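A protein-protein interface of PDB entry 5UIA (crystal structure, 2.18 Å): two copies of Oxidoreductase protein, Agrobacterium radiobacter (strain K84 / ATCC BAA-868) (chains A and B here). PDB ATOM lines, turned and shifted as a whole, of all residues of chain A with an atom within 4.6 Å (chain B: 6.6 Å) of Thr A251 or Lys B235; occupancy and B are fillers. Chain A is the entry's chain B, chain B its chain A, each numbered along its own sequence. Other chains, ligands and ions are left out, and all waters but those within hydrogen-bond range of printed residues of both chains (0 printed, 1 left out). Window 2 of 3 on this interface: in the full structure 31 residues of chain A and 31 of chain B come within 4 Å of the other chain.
The side-chain amino group (NZ) of Lys B235 is in hydrogen-bond range of the backbone carbonyl oxygen (O) of Thr A251 (3.4 Å).
N of Gly B237 is in hydrogen-bond range of OG1 of Thr A266, at 2.9 Å.
O of Lys B235 is in hydrogen-bond range of OG1 of Thr A254, 2.9 Å away.
N of Ala B233 is in hydrogen-bond range of O of Ser B157, at 3.3 Å.
N of Thr A251 sits at hydrogen-bond distance from O of Glu A147, at 2.9 Å.
N of Gly B158 sits at hydrogen-bond distance from O of Thr B234.
OG1 of Thr B234 is in hydrogen-bond range of OG of Ser B231 (2.6 Å).
O of Ile A145 is in hydrogen-bond range of N of Thr A251, 3.3 Å away.
The backbone NH (N) of Ala B233 is in hydrogen-bond range of the side-chain hydroxyl (OG) of Ser B231 (3.0 Å).
Among the printed residues, merely in contact across the chains: Thr A254 with Leu B236 (3.5 Å), Thr A266 with Lys B235 (3.5 Å), Phe A149 with Ala B233 (3.6 Å), Thr A266 with Leu B236 (3.7 Å), Phe A149 with Val B204 (3.7 Å), Thr A254 with Thr B234 (3.8 Å), Gly A253 with Lys B235 (3.9 Å) and Gln A252 with Lys B235 (3.9 Å).
Ile A145 touches none of the printed residues of chain B.
Of chain B, only Lys B235 (3.4 Å) comes within 4 Å of Thr A251.
Printed residues of chain B within 4 Å of Gln A252: Lys B235 (3.9 Å).
Printed residues of chain B within 4 Å of Thr A254: Thr B234, Lys B235 and Leu B236.
Printed residues of chain A within 4 Å of Ala B233: Phe A149.
Printed residues of chain A within 4 Å of Thr B234: Thr A254.
Lys B235 touches five residues of chain A.
Of the printed residues of chain A, Gly B237 touches Thr A266 (2.9 Å).
The nearest printed residue of chain A that does not touch Lys B235 is Gly A250 (5.1 Å).
The nearest printed residue of chain B that does not touch Thr A266 is Thr B234 (7.5 Å).
Of the 10 printed residues of chain B, 6 touch a printed residue of chain A.
Hydrophobic or aromatic side chains of chain B within 4 Å of the printed part of chain A: Val B204, Ala B233 and Leu B236.
Of the 10 printed residues of chain A, 6 touch a printed residue of chain B.
Printed residues of chain A that touch a printed residue of chain B: Phe A149, Thr A251, Gln A252, Gly A253, Thr A254 and Thr A266.
Hydrophobic or aromatic side chains of chain A that line the printed part of chain B: Phe A149.
Among the printed residues, no Asp or Glu carboxylate lies within 4 Å of a Lys or Arg side-chain nitrogen of the other chain.
No position is printed for both chains.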
ATOM      1  N   ILE A 145       3.809 -19.439  -6.960  1.00  0.00           N
ATOM      2  CA  ILE A 145       4.847 -20.448  -6.707  1.00  0.00           C
ATOM      3  C   ILE A 145       6.137 -20.254  -7.510  1.00  0.00           C
ATOM      4  O   ILE A 145       6.986 -21.158  -7.539  1.00  0.00           O
ATOM      5  CB  ILE A 145       4.319 -21.893  -6.886  1.00  0.00           C
ATOM      6  CG1 ILE A 145       3.927 -22.194  -8.327  1.00  0.00           C
ATOM      7  CG2 ILE A 145       3.151 -22.149  -5.945  1.00  0.00           C
ATOM      8  CD1 ILE A 145       3.838 -23.682  -8.606  1.00  0.00           C
ATOM      9  N   GLY A 146       6.316 -19.075  -8.105  1.00  0.00           N
ATOM     10  CA  GLY A 146       7.492 -18.793  -8.915  1.00  0.00           C
ATOM     11  C   GLY A 146       7.417 -19.502 -10.253  1.00  0.00           C
ATOM     12  O   GLY A 146       6.316 -19.731 -10.767  1.00  0.00           O
ATOM     13  N   GLU A 147       8.584 -19.833 -10.812  1.00  0.00           N
ATOM     14  CA  GLU A 147       8.680 -20.499 -12.117  1.00  0.00           C
ATOM     15  C   GLU A 147       8.519 -22.013 -11.939  1.00  0.00           C
ATOM     16  O   GLU A 147       9.215 -22.600 -11.112  1.00  0.00           O
ATOM     17  CB  GLU A 147      10.043 -20.230 -12.775  1.00  0.00           C
ATOM     18  CG  GLU A 147      10.363 -18.763 -13.041  1.00  0.00           C
ATOM     19  CD  GLU A 147       9.384 -18.089 -13.996  1.00  0.00           C
ATOM     20  OE1 GLU A 147       8.854 -18.752 -14.925  1.00  0.00           O
ATOM     21  OE2 GLU A 147       9.148 -16.877 -13.818  1.00  0.00           O
ATOM     22  N   PHE A 149       9.105 -25.884 -12.458  1.00  0.00           N
ATOM     23  CA  PHE A 149      10.153 -26.763 -13.007  1.00  0.00           C
ATOM     24  C   PHE A 149       9.800 -28.245 -13.117  1.00  0.00           C
ATOM     25  O   PHE A 149      10.497 -28.978 -13.813  1.00  0.00           O
ATOM     26  CB  PHE A 149      11.477 -26.589 -12.242  1.00  0.00           C
ATOM     27  CG  PHE A 149      11.429 -27.013 -10.804  1.00  0.00           C
ATOM     28  CD1 PHE A 149      11.560 -28.358 -10.449  1.00  0.00           C
ATOM     29  CD2 PHE A 149      11.276 -26.070  -9.798  1.00  0.00           C
ATOM     30  CE1 PHE A 149      11.534 -28.745  -9.114  1.00  0.00           C
ATOM     31  CE2 PHE A 149      11.238 -26.454  -8.466  1.00  0.00           C
ATOM     32  CZ  PHE A 149      11.373 -27.790  -8.119  1.00  0.00           C
ATOM     33  N   GLY A 250       7.481 -25.443  -8.156  1.00  0.00           N
ATOM     34  CA  GLY A 250       8.057 -24.216  -8.685  1.00  0.00           C
ATOM     35  C   GLY A 250       9.164 -23.714  -7.793  1.00  0.00           C
ATOM     36  O   GLY A 250       9.357 -24.230  -6.688  1.00  0.00           O
ATOM     37  N   THR A 251       9.868 -22.681  -8.259  1.00  0.00           N
ATOM     38  CA  THR A 251      10.985 -22.094  -7.516  1.00  0.00           C
ATOM     39  C   THR A 251      10.601 -21.567  -6.134  1.00  0.00           C
ATOM     40  O   THR A 251      11.454 -21.489  -5.258  1.00  0.00           O
ATOM     41  CB  THR A 251      11.671 -20.947  -8.299  1.00  0.00           C
ATOM     42  OG1 THR A 251      10.689 -20.004  -8.739  1.00  0.00           O
ATOM     43  CG2 THR A 251      12.418 -21.480  -9.517  1.00  0.00           C
ATOM     44  N   GLN A 252       9.333 -21.199  -5.934  1.00  0.00           N
ATOM     45  CA  GLN A 252       8.887 -20.595  -4.657  1.00  0.00           C
ATOM     46  C   GLN A 252       7.715 -21.319  -3.979  1.00  0.00           C
ATOM     47  O   GLN A 252       7.220 -20.855  -2.957  1.00  0.00           O
ATOM     48  CB  GLN A 252       8.527 -19.111  -4.873  1.00  0.00           C
ATOM     49  CG  GLN A 252       9.688 -18.225  -5.294  1.00  0.00           C
ATOM     50  CD  GLN A 252       9.222 -16.850  -5.789  1.00  0.00           C
ATOM     51  OE1 GLN A 252       8.254 -16.274  -5.274  1.00  0.00           O
ATOM     52  NE2 GLN A 252       9.900 -16.331  -6.805  1.00  0.00           N
ATOM     53  N   GLY A 253       7.273 -22.448  -4.517  1.00  0.00           N
ATOM     54  CA  GLY A 253       6.144 -23.150  -3.918  1.00  0.00           C
ATOM     55  C   GLY A 253       5.708 -24.386  -4.670  1.00  0.00           C
ATOM     56  O   GLY A 253       6.400 -24.842  -5.575  1.00  0.00           O
ATOM     57  N   THR A 254       4.549 -24.918  -4.290  1.00  0.00           N
ATOM     58  CA  THR A 254       3.956 -26.075  -4.957  1.00  0.00           C
ATOM     59  C   THR A 254       2.455 -25.897  -5.151  1.00  0.00           C
ATOM     60  O   THR A 254       1.820 -25.122  -4.446  1.00  0.00           O
ATOM     61  CB  THR A 254       4.160 -27.360  -4.139  1.00  0.00           C
ATOM     62  OG1 THR A 254       3.729 -27.138  -2.793  1.00  0.00           O
ATOM     63  CG2 THR A 254       5.621 -27.772  -4.118  1.00  0.00           C
ATOM     64  N   THR A 266       1.157 -23.988  -1.604  1.00  0.00           N
ATOM     65  CA  THR A 266       2.152 -23.517  -0.644  1.00  0.00           C
ATOM     66  C   THR A 266       3.022 -22.503  -1.367  1.00  0.00           C
ATOM     67  O   THR A 266       3.502 -22.778  -2.465  1.00  0.00           O
ATOM     68  CB  THR A 266       3.058 -24.666  -0.161  1.00  0.00           C
ATOM     69  OG1 THR A 266       2.254 -25.700   0.415  1.00  0.00           O
ATOM     70  CG2 THR A 266       4.076 -24.172   0.872  1.00  0.00           C
ATOM     71  N   SER B 157      11.264 -33.052  -1.159  1.00  0.00           N
ATOM     72  CA  SER B 157      11.499 -32.359   0.110  1.00  0.00           C
ATOM     73  C   SER B 157      12.069 -30.965  -0.123  1.00  0.00           C
ATOM     74  O   SER B 157      12.616 -30.691  -1.180  1.00  0.00           O
ATOM     75  CB  SER B 157      12.499 -33.166   0.946  1.00  0.00           C
ATOM     76  OG  SER B 157      12.796 -32.519   2.168  1.00  0.00           O
ATOM     77  N   GLY B 158      11.913 -30.093   0.875  1.00  0.00           N
ATOM     78  CA  GLY B 158      12.652 -28.830   0.975  1.00  0.00           C
ATOM     79  C   GLY B 158      13.483 -28.737   2.253  1.00  0.00           C
ATOM     80  O   GLY B 158      13.850 -27.644   2.663  1.00  0.00           O
ATOM     81  N   VAL B 204      17.905 -26.320  -9.423  1.00  0.00           N
ATOM     82  CA  VAL B 204      17.022 -25.201  -9.063  1.00  0.00           C
ATOM     83  C   VAL B 204      17.674 -24.297  -8.006  1.00  0.00           C
ATOM     84  O   VAL B 204      17.684 -23.082  -8.149  1.00  0.00           O
ATOM     85  CB  VAL B 204      15.666 -25.728  -8.528  1.00  0.00           C
ATOM     86  CG1 VAL B 204      14.761 -24.577  -8.081  1.00  0.00           C
ATOM     87  CG2 VAL B 204      14.982 -26.578  -9.588  1.00  0.00           C
ATOM     88  N   SER B 231      13.580 -34.822  -5.297  1.00  0.00           N
ATOM     89  CA  SER B 231      13.759 -33.367  -5.304  1.00  0.00           C
ATOM     90  C   SER B 231      14.101 -32.861  -3.922  1.00  0.00           C
ATOM     91  O   SER B 231      13.463 -33.265  -2.944  1.00  0.00           O
ATOM     92  CB  SER B 231      12.482 -32.650  -5.797  1.00  0.00           C
ATOM     93  OG  SER B 231      12.560 -31.232  -5.605  1.00  0.00           O
ATOM     94  N   ALA B 233      14.152 -29.399  -3.852  1.00  0.00           N
ATOM     95  CA  ALA B 233      13.690 -28.029  -4.144  1.00  0.00           C
ATOM     96  C   ALA B 233      12.159 -27.902  -4.090  1.00  0.00           C
ATOM     97  O   ALA B 233      11.582 -26.955  -4.621  1.00  0.00           O
ATOM     98  CB  ALA B 233      14.207 -27.597  -5.499  1.00  0.00           C
ATOM     99  N   THR B 234      11.515 -28.835  -3.398  1.00  0.00           N
ATOM    100  CA  THR B 234      10.067 -28.912  -3.327  1.00  0.00           C
ATOM    101  C   THR B 234       9.600 -28.325  -1.987  1.00  0.00           C
ATOM    102  O   THR B 234       9.939 -28.846  -0.913  1.00  0.00           O
ATOM    103  CB  THR B 234       9.629 -30.372  -3.508  1.00  0.00           C
ATOM    104  OG1 THR B 234      10.132 -30.835  -4.766  1.00  0.00           O
ATOM    105  CG2 THR B 234       8.110 -30.523  -3.492  1.00  0.00           C
ATOM    106  N   LYS B 235       8.827 -27.238  -2.070  1.00  0.00           N
ATOM    107  CA  LYS B 235       8.362 -26.478  -0.908  1.00  0.00           C
ATOM    108  C   LYS B 235       6.901 -26.784  -0.644  1.00  0.00           C
ATOM    109  O   LYS B 235       5.997 -26.247  -1.310  1.00  0.00           O
ATOM    110  CB  LYS B 235       8.581 -24.975  -1.118  1.00  0.00           C
ATOM    111  CG  LYS B 235      10.062 -24.633  -1.237  1.00  0.00           C
ATOM    112  CD  LYS B 235      10.355 -23.253  -1.832  1.00  0.00           C
ATOM    113  CE  LYS B 235      11.799 -23.203  -2.339  1.00  0.00           C
ATOM    114  NZ  LYS B 235      12.466 -21.912  -2.047  1.00  0.00           N
ATOM    115  N   LEU B 236       6.683 -27.666   0.326  1.00  0.00           N
ATOM    116  CA  LEU B 236       5.354 -28.110   0.718  1.00  0.00           C
ATOM    117  C   LEU B 236       4.981 -27.526   2.076  1.00  0.00           C
ATOM    118  O   LEU B 236       5.852 -27.192   2.874  1.00  0.00           O
ATOM    119  CB  LEU B 236       5.330 -29.631   0.761  1.00  0.00           C
ATOM    120  CG  LEU B 236       5.384 -30.316  -0.606  1.00  0.00           C
ATOM    121  CD1 LEU B 236       5.898 -31.746  -0.461  1.00  0.00           C
ATOM    122  CD2 LEU B 236       4.013 -30.291  -1.277  1.00  0.00           C
ATOM    123  N   GLY B 237       3.687 -27.394   2.326  1.00  0.00           N
ATOM    124  CA  GLY B 237       3.197 -26.831   3.580  1.00  0.00           C
ATOM    125  C   GLY B 237       3.544 -27.706   4.760  1.00  0.00           C
ATOM    126  O   GLY B 237       3.876 -27.209   5.830  1.00  0.00           O
ATOM    127  N   GLU B 239       6.327 -30.497   5.567  1.00  0.00           N
ATOM    128  CA  GLU B 239       7.582 -31.069   5.101  1.00  0.00           C
ATOM    129  C   GLU B 239       7.522 -32.594   5.315  1.00  0.00           C
ATOM    130  O   GLU B 239       7.337 -33.027   6.442  1.00  0.00           O
ATOM    131  CB  GLU B 239       8.754 -30.432   5.877  1.00  0.00           C
ATOM    132  CG  GLU B 239      10.146 -30.982   5.579  1.00  0.00           C
ATOM    133  CD  GLU B 239      10.479 -31.068   4.091  1.00  0.00           C
ATOM    134  OE1 GLU B 239      10.570 -30.004   3.436  1.00  0.00           O
ATOM    135  OE2 GLU B 239      10.680 -32.202   3.578  1.00  0.00           O
